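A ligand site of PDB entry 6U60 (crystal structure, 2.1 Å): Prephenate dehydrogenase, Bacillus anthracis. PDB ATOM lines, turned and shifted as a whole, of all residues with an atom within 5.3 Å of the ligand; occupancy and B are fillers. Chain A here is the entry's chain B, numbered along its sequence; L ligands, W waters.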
ATOM      1  N   ILE A  23      -3.586   7.442  28.893  1.00  0.00           N
ATOM      2  CA  ILE A  23      -3.602   8.665  29.752  1.00  0.00           C
ATOM      3  C   ILE A  23      -3.270   9.863  28.868  1.00  0.00           C
ATOM      4  O   ILE A  23      -2.104   9.973  28.421  1.00  0.00           O
ATOM      5  CB  ILE A  23      -2.594   8.493  30.910  1.00  0.00           C
ATOM      6  CG1 ILE A  23      -2.998   7.318  31.818  1.00  0.00           C
ATOM      7  CG2 ILE A  23      -2.435   9.797  31.678  1.00  0.00           C
ATOM      8  CD1 ILE A  23      -1.956   6.928  32.835  1.00  0.00           C
ATOM      9  N   GLY A  24      -4.257  10.712  28.588  1.00  0.00           N
ATOM     10  CA  GLY A  24      -4.188  11.805  27.602  1.00  0.00           C
ATOM     11  C   GLY A  24      -4.750  11.328  26.267  1.00  0.00           C
ATOM     12  O   GLY A  24      -3.974  10.741  25.500  1.00  0.00           O
ATOM     13  N   THR A  25      -6.034  11.536  26.008  1.00  0.00           N
ATOM     14  CA  THR A  25      -6.734  11.009  24.801  1.00  0.00           C
ATOM     15  C   THR A  25      -6.827  12.143  23.784  1.00  0.00           C
ATOM     16  O   THR A  25      -7.929  12.633  23.534  1.00  0.00           O
ATOM     17  CB  THR A  25      -8.085  10.376  25.163  1.00  0.00           C
ATOM     18  OG1 THR A  25      -8.953  11.380  25.697  1.00  0.00           O
ATOM     19  CG2 THR A  25      -7.972   9.289  26.211  1.00  0.00           C
ATOM     20  N   GLY A  26      -5.671  12.590  23.290  1.00  0.00           N
ATOM     21  CA  GLY A  26      -5.589  13.643  22.262  1.00  0.00           C
ATOM     22  C   GLY A  26      -5.227  13.067  20.896  1.00  0.00           C
ATOM     23  O   GLY A  26      -5.655  11.940  20.573  1.00  0.00           O
ATOM     24  N   LEU A  27      -4.480  13.839  20.113  1.00  0.00           N
ATOM     25  CA  LEU A  27      -4.141  13.513  18.706  1.00  0.00           C
ATOM     26  C   LEU A  27      -3.281  12.247  18.713  1.00  0.00           C
ATOM     27  O   LEU A  27      -3.646  11.248  18.089  1.00  0.00           O
ATOM     28  CB  LEU A  27      -3.355  14.684  18.127  1.00  0.00           C
ATOM     29  CG  LEU A  27      -2.705  14.417  16.772  1.00  0.00           C
ATOM     30  CD1 LEU A  27      -3.798  14.343  15.706  1.00  0.00           C
ATOM     31  CD2 LEU A  27      -1.644  15.486  16.462  1.00  0.00           C
ATOM     32  N   ILE A  28      -2.136  12.349  19.367  1.00  0.00           N
ATOM     33  CA  ILE A  28      -1.099  11.298  19.366  1.00  0.00           C
ATOM     34  C   ILE A  28      -1.637  10.090  20.150  1.00  0.00           C
ATOM     35  O   ILE A  28      -1.598   8.987  19.608  1.00  0.00           O
ATOM     36  CB  ILE A  28       0.220  11.854  19.913  1.00  0.00           C
ATOM     37  CG1 ILE A  28       0.730  13.046  19.106  1.00  0.00           C
ATOM     38  CG2 ILE A  28       1.264  10.754  20.047  1.00  0.00           C
ATOM     39  CD1 ILE A  28       1.065  12.693  17.688  1.00  0.00           C
ATOM     40  N   GLY A  29      -2.113  10.275  21.387  1.00  0.00           N
ATOM     41  CA  GLY A  29      -2.762   9.201  22.167  1.00  0.00           C
ATOM     42  C   GLY A  29      -3.821   8.453  21.358  1.00  0.00           C
ATOM     43  O   GLY A  29      -3.765   7.201  21.244  1.00  0.00           O
ATOM     44  N   TYR A  47      -8.307   7.887  29.955  1.00  0.00           N
ATOM     45  CA  TYR A  47      -8.238   8.837  31.097  1.00  0.00           C
ATOM     46  C   TYR A  47      -7.724  10.179  30.573  1.00  0.00           C
ATOM     47  O   TYR A  47      -6.664  10.233  29.873  1.00  0.00           O
ATOM     48  CB  TYR A  47      -7.322   8.287  32.196  1.00  0.00           C
ATOM     49  CG  TYR A  47      -7.026   9.260  33.309  1.00  0.00           C
ATOM     50  CD1 TYR A  47      -5.985  10.161  33.201  1.00  0.00           C
ATOM     51  CD2 TYR A  47      -7.815   9.313  34.459  1.00  0.00           C
ATOM     52  CE1 TYR A  47      -5.696  11.063  34.213  1.00  0.00           C
ATOM     53  CE2 TYR A  47      -7.560  10.228  35.471  1.00  0.00           C
ATOM     54  CZ  TYR A  47      -6.483  11.092  35.358  1.00  0.00           C
ATOM     55  OH  TYR A  47      -6.189  11.991  36.329  1.00  0.00           O
ATOM     56  N   ASP A  48      -8.453  11.243  30.880  1.00  0.00           N
ATOM     57  CA  ASP A  48      -8.045  12.597  30.452  1.00  0.00           C
ATOM     58  C   ASP A  48      -8.489  13.614  31.501  1.00  0.00           C
ATOM     59  O   ASP A  48      -9.578  13.460  32.058  1.00  0.00           O
ATOM     60  CB  ASP A  48      -8.563  12.926  29.058  1.00  0.00           C
ATOM     61  CG  ASP A  48      -7.748  14.040  28.390  1.00  0.00           C
ATOM     62  OD1 ASP A  48      -7.853  15.177  28.833  1.00  0.00           O
ATOM     63  OD2 ASP A  48      -6.981  13.717  27.464  1.00  0.00           O
ATOM     64  N   ILE A  49      -7.645  14.625  31.700  1.00  0.00           N
ATOM     65  CA  ILE A  49      -7.899  15.744  32.640  1.00  0.00           C
ATOM     66  C   ILE A  49      -9.112  16.524  32.113  1.00  0.00           C
ATOM     67  O   ILE A  49      -9.888  17.028  32.958  1.00  0.00           O
ATOM     68  CB  ILE A  49      -6.612  16.584  32.811  1.00  0.00           C
ATOM     69  CG1 ILE A  49      -6.667  17.466  34.058  1.00  0.00           C
ATOM     70  CG2 ILE A  49      -6.302  17.383  31.556  1.00  0.00           C
ATOM     71  CD1 ILE A  49      -5.517  18.454  34.175  1.00  0.00           C
ATOM     72  N   PHE A  50      -9.308  16.601  30.799  1.00  0.00           N
ATOM     73  CA  PHE A  50     -10.521  17.227  30.200  1.00  0.00           C
ATOM     74  C   PHE A  50     -11.550  16.122  29.879  1.00  0.00           C
ATOM     75  O   PHE A  50     -11.422  15.419  28.842  1.00  0.00           O
ATOM     76  CB  PHE A  50     -10.135  18.114  28.999  1.00  0.00           C
ATOM     77  CG  PHE A  50      -9.557  19.444  29.429  1.00  0.00           C
ATOM     78  CD1 PHE A  50     -10.354  20.412  30.021  1.00  0.00           C
ATOM     79  CD2 PHE A  50      -8.198  19.708  29.286  1.00  0.00           C
ATOM     80  CE1 PHE A  50      -9.820  21.623  30.433  1.00  0.00           C
ATOM     81  CE2 PHE A  50      -7.653  20.910  29.706  1.00  0.00           C
ATOM     82  CZ  PHE A  50      -8.469  21.872  30.275  1.00  0.00           C
ATOM     83  N   GLN A  53     -13.026  15.334  26.345  1.00  0.00           N
ATOM     84  CA  GLN A  53     -12.081  14.754  25.331  1.00  0.00           C
ATOM     85  C   GLN A  53     -12.205  13.228  25.363  1.00  0.00           C
ATOM     86  O   GLN A  53     -12.363  12.607  24.302  1.00  0.00           O
ATOM     87  CB  GLN A  53     -10.630  15.161  25.613  1.00  0.00           C
ATOM     88  CG  GLN A  53     -10.370  16.660  25.656  1.00  0.00           C
ATOM     89  CD  GLN A  53     -10.772  17.387  24.383  1.00  0.00           C
ATOM     90  OE1 GLN A  53     -10.496  16.922  23.267  1.00  0.00           O
ATOM     91  NE2 GLN A  53     -11.432  18.519  24.568  1.00  0.00           N
ATOM     92  N   ALA A  83       0.184   9.873  26.878  1.00  0.00           N
ATOM     93  CA  ALA A  83       0.115  10.752  25.687  1.00  0.00           C
ATOM     94  C   ALA A  83      -0.283  12.170  26.134  1.00  0.00           C
ATOM     95  O   ALA A  83      -0.767  12.965  25.317  1.00  0.00           O
ATOM     96  CB  ALA A  83      -0.837  10.113  24.695  1.00  0.00           C
ATOM     97  N   SER A  84      -0.088  12.467  27.434  1.00  0.00           N
ATOM     98  CA  SER A  84      -0.188  13.818  28.040  1.00  0.00           C
ATOM     99  C   SER A  84       1.087  14.600  27.708  1.00  0.00           C
ATOM    100  O   SER A  84       2.089  14.002  27.282  1.00  0.00           O
ATOM    101  CB  SER A  84      -0.360  13.673  29.527  1.00  0.00           C
ATOM    102  OG  SER A  84       0.514  12.652  29.991  1.00  0.00           O
ATOM    103  N   PRO A  85       1.110  15.940  27.853  1.00  0.00           N
ATOM    104  CA  PRO A  85       2.344  16.688  27.654  1.00  0.00           C
ATOM    105  C   PRO A  85       3.429  16.198  28.630  1.00  0.00           C
ATOM    106  O   PRO A  85       3.066  15.675  29.684  1.00  0.00           O
ATOM    107  CB  PRO A  85       1.975  18.161  27.877  1.00  0.00           C
ATOM    108  CG  PRO A  85       0.458  18.212  27.895  1.00  0.00           C
ATOM    109  CD  PRO A  85      -0.039  16.802  28.156  1.00  0.00           C
ATOM    110  N   VAL A  86       4.702  16.351  28.264  1.00  0.00           N
ATOM    111  CA  VAL A  86       5.856  15.736  28.987  1.00  0.00           C
ATOM    112  C   VAL A  86       5.855  16.211  30.436  1.00  0.00           C
ATOM    113  O   VAL A  86       6.113  15.370  31.332  1.00  0.00           O
ATOM    114  CB  VAL A  86       7.199  16.036  28.297  1.00  0.00           C
ATOM    115  CG1 VAL A  86       8.377  15.879  29.255  1.00  0.00           C
ATOM    116  CG2 VAL A  86       7.399  15.185  27.055  1.00  0.00           C
ATOM    117  N   GLU A  88       3.321  17.007  32.257  1.00  0.00           N
ATOM    118  CA  GLU A  88       2.196  16.322  32.953  1.00  0.00           C
ATOM    119  C   GLU A  88       2.544  14.847  33.173  1.00  0.00           C
ATOM    120  O   GLU A  88       2.262  14.357  34.279  1.00  0.00           O
ATOM    121  CB  GLU A  88       0.880  16.496  32.165  1.00  0.00           C
ATOM    122  CG  GLU A  88       0.496  17.949  32.008  1.00  0.00           C
ATOM    123  CD  GLU A  88       0.299  18.612  33.364  1.00  0.00           C
ATOM    124  OE1 GLU A  88      -0.464  18.044  34.149  1.00  0.00           O
ATOM    125  OE2 GLU A  88       0.956  19.622  33.649  1.00  0.00           O
ATOM    126  N   LEU A  92       2.629  12.564  36.689  1.00  0.00           N
ATOM    127  CA  LEU A  92       1.758  11.380  36.885  1.00  0.00           C
ATOM    128  C   LEU A  92       2.579  10.115  37.160  1.00  0.00           C
ATOM    129  O   LEU A  92       1.980   9.184  37.753  1.00  0.00           O
ATOM    130  CB  LEU A  92       0.865  11.182  35.660  1.00  0.00           C
ATOM    131  CG  LEU A  92      -0.106  12.322  35.384  1.00  0.00           C
ATOM    132  CD1 LEU A  92      -0.560  12.295  33.944  1.00  0.00           C
ATOM    133  CD2 LEU A  92      -1.288  12.235  36.323  1.00  0.00           C
ATOM    134  N   VAL A 110       4.928   9.227  24.809  1.00  0.00           N
ATOM    135  CA  VAL A 110       5.078   9.676  23.403  1.00  0.00           C
ATOM    136  C   VAL A 110       5.820  11.017  23.374  1.00  0.00           C
ATOM    137  O   VAL A 110       5.855  11.630  22.291  1.00  0.00           O
ATOM    138  CB  VAL A 110       3.692   9.760  22.718  1.00  0.00           C
ATOM    139  CG1 VAL A 110       3.019   8.407  22.666  1.00  0.00           C
ATOM    140  CG2 VAL A 110       2.790  10.764  23.388  1.00  0.00           C
ATOM    141  N   GLY A 111       6.406  11.456  24.487  1.00  0.00           N
ATOM    142  CA  GLY A 111       7.098  12.779  24.574  1.00  0.00           C
ATOM    143  C   GLY A 111       8.117  13.060  23.476  1.00  0.00           C
ATOM    144  O   GLY A 111       8.935  12.161  23.185  1.00  0.00           O
ATOM    145  N   SER A 112       8.150  14.286  22.986  1.00  0.00           N
ATOM    146  CA  SER A 112       9.120  14.822  21.987  1.00  0.00           C
ATOM    147  C   SER A 112      10.545  14.899  22.576  1.00  0.00           C
ATOM    148  O   SER A 112      11.518  14.960  21.788  1.00  0.00           O
ATOM    149  CB  SER A 112       8.687  16.197  21.499  1.00  0.00           C
ATOM    150  OG  SER A 112       7.438  16.141  20.823  1.00  0.00           O
ATOM    151  N   HIS A 135       8.785   8.052  21.314  1.00  0.00           N
ATOM    152  CA  HIS A 135       8.636   9.324  20.578  1.00  0.00           C
ATOM    153  C   HIS A 135       8.282   8.975  19.147  1.00  0.00           C
ATOM    154  O   HIS A 135       9.192   8.796  18.343  1.00  0.00           O
ATOM    155  CB  HIS A 135       9.927  10.163  20.671  1.00  0.00           C
ATOM    156  CG  HIS A 135       9.857  11.430  19.889  1.00  0.00           C
ATOM    157  ND1 HIS A 135      10.967  12.165  19.575  1.00  0.00           N
ATOM    158  CD2 HIS A 135       8.819  12.073  19.319  1.00  0.00           C
ATOM    159  CE1 HIS A 135      10.622  13.202  18.852  1.00  0.00           C
ATOM    160  NE2 HIS A 135       9.297  13.198  18.727  1.00  0.00           N
ATOM    161  N   PRO A 136       6.987   8.917  18.787  1.00  0.00           N
ATOM    162  CA  PRO A 136       6.579   8.823  17.388  1.00  0.00           C
ATOM    163  C   PRO A 136       6.799  10.163  16.677  1.00  0.00           C
ATOM    164  O   PRO A 136       6.286  11.152  17.150  1.00  0.00           O
ATOM    165  CB  PRO A 136       5.082   8.495  17.435  1.00  0.00           C
ATOM    166  CG  PRO A 136       4.615   8.914  18.799  1.00  0.00           C
ATOM    167  CD  PRO A 136       5.840   9.033  19.678  1.00  0.00           C
ATOM    168  N   MET A 137       7.565  10.185  15.594  1.00  0.00           N
ATOM    169  CA  MET A 137       7.892  11.440  14.874  1.00  0.00           C
ATOM    170  C   MET A 137       6.864  11.648  13.753  1.00  0.00           C
ATOM    171  O   MET A 137       7.105  11.270  12.604  1.00  0.00           O
ATOM    172  CB  MET A 137       9.316  11.396  14.342  1.00  0.00           C
ATOM    173  CG  MET A 137      10.343  11.395  15.459  1.00  0.00           C
ATOM    174  SD  MET A 137      12.022  11.220  14.793  1.00  0.00           S
ATOM    175  CE  MET A 137      12.902  11.901  16.194  1.00  0.00           C
ATOM    176  N   ALA A 138       5.702  12.101  14.169  1.00  0.00           N
ATOM    177  CA  ALA A 138       4.572  12.431  13.275  1.00  0.00           C
ATOM    178  C   ALA A 138       3.820  13.600  13.900  1.00  0.00           C
ATOM    179  O   ALA A 138       3.818  13.676  15.130  1.00  0.00           O
ATOM    180  CB  ALA A 138       3.700  11.235  13.102  1.00  0.00           C
ATOM    181  N   GLY A 139       3.267  14.480  13.077  1.00  0.00           N
ATOM    182  CA  GLY A 139       2.521  15.644  13.553  1.00  0.00           C
ATOM    183  C   GLY A 139       1.221  15.833  12.822  1.00  0.00           C
ATOM    184  O   GLY A 139       0.772  14.938  12.071  1.00  0.00           O
ATOM    185  N   SER A 140       0.614  16.988  13.030  1.00  0.00           N
ATOM    186  CA  SER A 140      -0.694  17.343  12.445  1.00  0.00           C
ATOM    187  C   SER A 140      -0.856  18.853  12.550  1.00  0.00           C
ATOM    188  O   SER A 140      -0.220  19.434  13.423  1.00  0.00           O
ATOM    189  CB  SER A 140      -1.815  16.620  13.164  1.00  0.00           C
ATOM    190  OG  SER A 140      -3.049  16.860  12.509  1.00  0.00           O
ATOM    191  N   THR A 143      -4.528  19.604  16.992  1.00  0.00           N
ATOM    192  CA  THR A 143      -4.492  18.774  18.226  1.00  0.00           C
ATOM    193  C   THR A 143      -5.919  18.291  18.527  1.00  0.00           C
ATOM    194  O   THR A 143      -6.869  18.705  17.823  1.00  0.00           O
ATOM    195  CB  THR A 143      -3.805  19.510  19.373  1.00  0.00           C
ATOM    196  OG1 THR A 143      -4.630  20.623  19.664  1.00  0.00           O
ATOM    197  CG2 THR A 143      -2.414  19.988  19.016  1.00  0.00           C
ATOM    198  N   GLY A 144      -6.039  17.321  19.437  1.00  0.00           N
ATOM    199  CA  GLY A 144      -7.342  16.795  19.875  1.00  0.00           C
ATOM    200  C   GLY A 144      -7.686  15.482  19.214  1.00  0.00           C
ATOM    201  O   GLY A 144      -7.196  15.236  18.092  1.00  0.00           O
ATOM    202  N   VAL A 145      -8.516  14.689  19.888  1.00  0.00           N
ATOM    203  CA  VAL A 145      -8.843  13.280  19.526  1.00  0.00           C
ATOM    204  C   VAL A 145      -9.659  13.232  18.236  1.00  0.00           C
ATOM    205  O   VAL A 145      -9.662  12.195  17.575  1.00  0.00           O
ATOM    206  CB  VAL A 145      -9.577  12.589  20.685  1.00  0.00           C
ATOM    207  CG1 VAL A 145     -10.981  13.132  20.887  1.00  0.00           C
ATOM    208  CG2 VAL A 145      -9.585  11.078  20.499  1.00  0.00           C
ATOM    209  N   MET A 246       3.797  23.713  23.720  1.00  0.00           N
ATOM    210  CA  MET A 246       4.597  22.501  23.460  1.00  0.00           C
ATOM    211  C   MET A 246       6.080  22.873  23.219  1.00  0.00           C
ATOM    212  O   MET A 246       6.947  22.231  23.817  1.00  0.00           O
ATOM    213  CB  MET A 246       4.050  21.727  22.246  1.00  0.00           C
ATOM    214  CG  MET A 246       4.831  20.469  22.009  1.00  0.00           C
ATOM    215  SD  MET A 246       4.030  19.370  20.822  1.00  0.00           S
ATOM    216  CE  MET A 246       4.705  20.028  19.313  1.00  0.00           C
HETATM  217  P1  LIG L   1      -3.307  16.955  22.465  1.00  0.00           P
HETATM  218  O1  LIG L   1      -3.570  18.285  23.069  1.00  0.00           O
HETATM  219  O2  LIG L   1      -4.086  16.477  21.220  1.00  0.00           O
HETATM  220  O3  LIG L   1      -3.398  15.685  23.498  1.00  0.00           O
HETATM  221  C1  LIG L   1      -2.883  15.793  24.836  1.00  0.00           C
HETATM  222  C2  LIG L   1      -3.999  15.370  25.748  1.00  0.00           C
HETATM  223  O4  LIG L   1      -3.491  15.237  27.087  1.00  0.00           O
HETATM  224  C3  LIG L   1      -5.195  16.328  25.810  1.00  0.00           C
HETATM  225  O5  LIG L   1      -6.388  15.598  25.545  1.00  0.00           O
HETATM  226  C4  LIG L   1      -5.097  16.910  27.232  1.00  0.00           C
HETATM  227  O6  LIG L   1      -6.360  17.232  27.803  1.00  0.00           O
HETATM  228  C5  LIG L   1      -4.463  15.739  27.975  1.00  0.00           C
HETATM  229  N1  LIG L   1      -3.806  16.062  29.241  1.00  0.00           N
HETATM  230  C6  LIG L   1      -3.120  17.199  29.560  1.00  0.00           C
HETATM  231  N2  LIG L   1      -2.706  17.246  30.804  1.00  0.00           N
HETATM  232  C7  LIG L   1      -3.143  16.041  31.344  1.00  0.00           C
HETATM  233  C8  LIG L   1      -3.038  15.471  32.625  1.00  0.00           C
HETATM  234  N3  LIG L   1      -2.377  16.029  33.645  1.00  0.00           N
HETATM  235  N4  LIG L   1      -3.622  14.272  32.832  1.00  0.00           N
HETATM  236  C9  LIG L   1      -4.241  13.676  31.820  1.00  0.00           C
HETATM  237  N5  LIG L   1      -4.386  14.110  30.562  1.00  0.00           N
HETATM  238  C10 LIG L   1      -3.821  15.304  30.384  1.00  0.00           C
HETATM  239  O7  LIG L   1      -1.751  16.904  22.126  1.00  0.00           O
HETATM  240  P2  LIG L   1      -0.900  15.868  21.256  1.00  0.00           P
HETATM  241  O8  LIG L   1      -1.607  14.569  21.210  1.00  0.00           O
HETATM  242  O9  LIG L   1      -0.467  16.509  19.989  1.00  0.00           O
HETATM  243  O10 LIG L   1       0.445  15.837  22.103  1.00  0.00           O
HETATM  244  C11 LIG L   1       0.677  15.012  23.256  1.00  0.00           C
HETATM  245  C12 LIG L   1       2.174  14.956  23.413  1.00  0.00           C
HETATM  246  O11 LIG L   1       2.704  14.116  22.376  1.00  0.00           O
HETATM  247  C13 LIG L   1       2.875  16.303  23.217  1.00  0.00           C
HETATM  248  O12 LIG L   1       3.014  17.039  24.419  1.00  0.00           O
HETATM  249  C14 LIG L   1       4.263  15.906  22.678  1.00  0.00           C
HETATM  250  O13 LIG L   1       5.256  15.839  23.691  1.00  0.00           O
HETATM  251  C15 LIG L   1       4.023  14.507  22.086  1.00  0.00           C
HETATM  252  N6  LIG L   1       4.187  14.537  20.582  1.00  0.00           N
HETATM  253  C16 LIG L   1       3.425  15.420  19.908  1.00  0.00           C
HETATM  254  C17 LIG L   1       3.598  15.589  18.546  1.00  0.00           C
HETATM  255  C18 LIG L   1       2.731  16.531  17.769  1.00  0.00           C
HETATM  256  O14 LIG L   1       3.048  16.841  16.620  1.00  0.00           O
HETATM  257  N7  LIG L   1       1.708  17.087  18.379  1.00  0.00           N
HETATM  258  C19 LIG L   1       4.560  14.818  17.900  1.00  0.00           C
HETATM  259  C20 LIG L   1       5.301  13.895  18.614  1.00  0.00           C
HETATM  260  C21 LIG L   1       5.109  13.772  19.967  1.00  0.00           C
HETATM  261  O   HOH W   1       5.921  16.412  15.298  1.00  0.00           O
HETATM  262  O   HOH W   2       1.710  19.567  24.200  1.00  0.00           O
HETATM  263  O   HOH W   3       5.286  17.932  25.779  1.00  0.00           O
HETATM  264  O   HOH W   4       0.752  18.803  20.343  1.00  0.00           O
HETATM  265  O   HOH W   5       7.734  14.823  17.132  1.00  0.00           O
HETATM  266  O   HOH W   6      -2.537  19.620  27.176  1.00  0.00           O
HETATM  267  O   HOH W   7      -2.433  19.723  32.059  1.00  0.00           O
HETATM  268  O   HOH W   8       0.084  18.562  16.232  1.00  0.00           O
HETATM  269  O   HOH W   9      -7.101  19.046  26.088  1.00  0.00           O
HETATM  270  O   HOH W  10      -4.354  14.102  35.385  1.00  0.00           O
HETATM  271  O   HOH W  11       2.305  18.594  14.736  1.00  0.00           O
HETATM  272  O   HOH W  12      -2.518  12.665  23.024  1.00  0.00           O
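Water W4 lies within hydrogen-bond range of O9 of the ligand (2.6 Å) and SD of Met 246 (3.4 Å).
Water W11 bridges O14 of the ligand (2.7 Å) and N of Ser 140 (2.9 Å).
Water W7 lies within hydrogen-bond range of a nitrogen (N2) of the ligand (2.8 Å) and the side-chain carboxylate of Glu 88 (3.3 Å).
Water W3 lies within hydrogen-bond range of an oxygen (O12) of the ligand (2.8 Å) and the backbone NH (N) of Val 86 (3.0 Å).
Water W8 bridges the backbone carbonyl oxygen (O) of Ser 140 and a nitrogen (N7) of the ligand.
Water W1 lies within hydrogen-bond range of O14 of the ligand (3.2 Å) and O of Ala 138 (3.5 Å).
OD1 of Asp 48 lies within hydrogen-bond range of O6 of the ligand (2.7 Å).
An oxygen (O2) of the ligand is in hydrogen-bond range of the backbone NH (N) of Gly 144 (2.8 Å).
The side-chain carboxylate (OE1) of Glu 88 lies within hydrogen-bond range of a nitrogen (N3) of the ligand, 2.8 Å away.
An oxygen (O2) of the ligand lies within hydrogen-bond range of the backbone NH of Leu 27 (2.9 Å).
An oxygen (O8) of the ligand lies within hydrogen-bond range of the backbone NH of Ile 28.
O13 of the ligand sits at hydrogen-bond distance from N of Ser 112, 3.4 Å away.
The backbone NH (N) of Ile 49 is in hydrogen-bond range of a nitrogen (N5) of the ligand (3.5 Å).
Gly 24 touches the ligand.
O of Thr 25 touches O5 of the ligand (3.9 Å).
Gly 26 touches the ligand (CA to O3, 3.2 Å).
CE1 of Tyr 47 touches C9 of the ligand (3.8 Å).
Phe 50 touches the ligand (CD2 to O6, 3.4 Å).
Ala 83 touches the ligand (O to C11, 3.2 Å).
Ser 84 touches the ligand (CA to O4, 3.7 Å).
Pro 85 touches the ligand.
Leu 92 touches the ligand.
Val 110 touches the ligand.
CA of Gly 111 touches O13 of the ligand, 3.7 Å away.
Pro 136 touches the ligand.
Ala 138 touches the ligand (O to C19, 3.1 Å).
Gly 139 touches the ligand (CA to O14, 3.3 Å).
Thr 143 touches the ligand.
SD of Met 246 touches C14 of the ligand, 3.9 Å away.
Hydrophobic or aromatic side chains within 4 Å of the ligand: Leu 27, Ile 28, Tyr 47, Ile 49, Phe 50, Pro 85, Leu 92, Val 110 and Met 246.
The nearest printed residue that does not touch the ligand is His 135 (4.02 Å).
OD1 of Asp 48 lies within hydrogen-bond range of N of Phe 50.
The side-chain carboxylate (OD2) of Asp 48 is in hydrogen-bond range of the backbone NH (N) of Thr 25 (2.8 Å).
N of Ala 83 lies within hydrogen-bond range of O of Ile 23.
The backbone NH of Gly 24 is in hydrogen-bond range of the backbone carbonyl oxygen of Tyr 47, 2.8 Å away.
N of Ser 84 lies within hydrogen-bond range of O of Ile 23.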
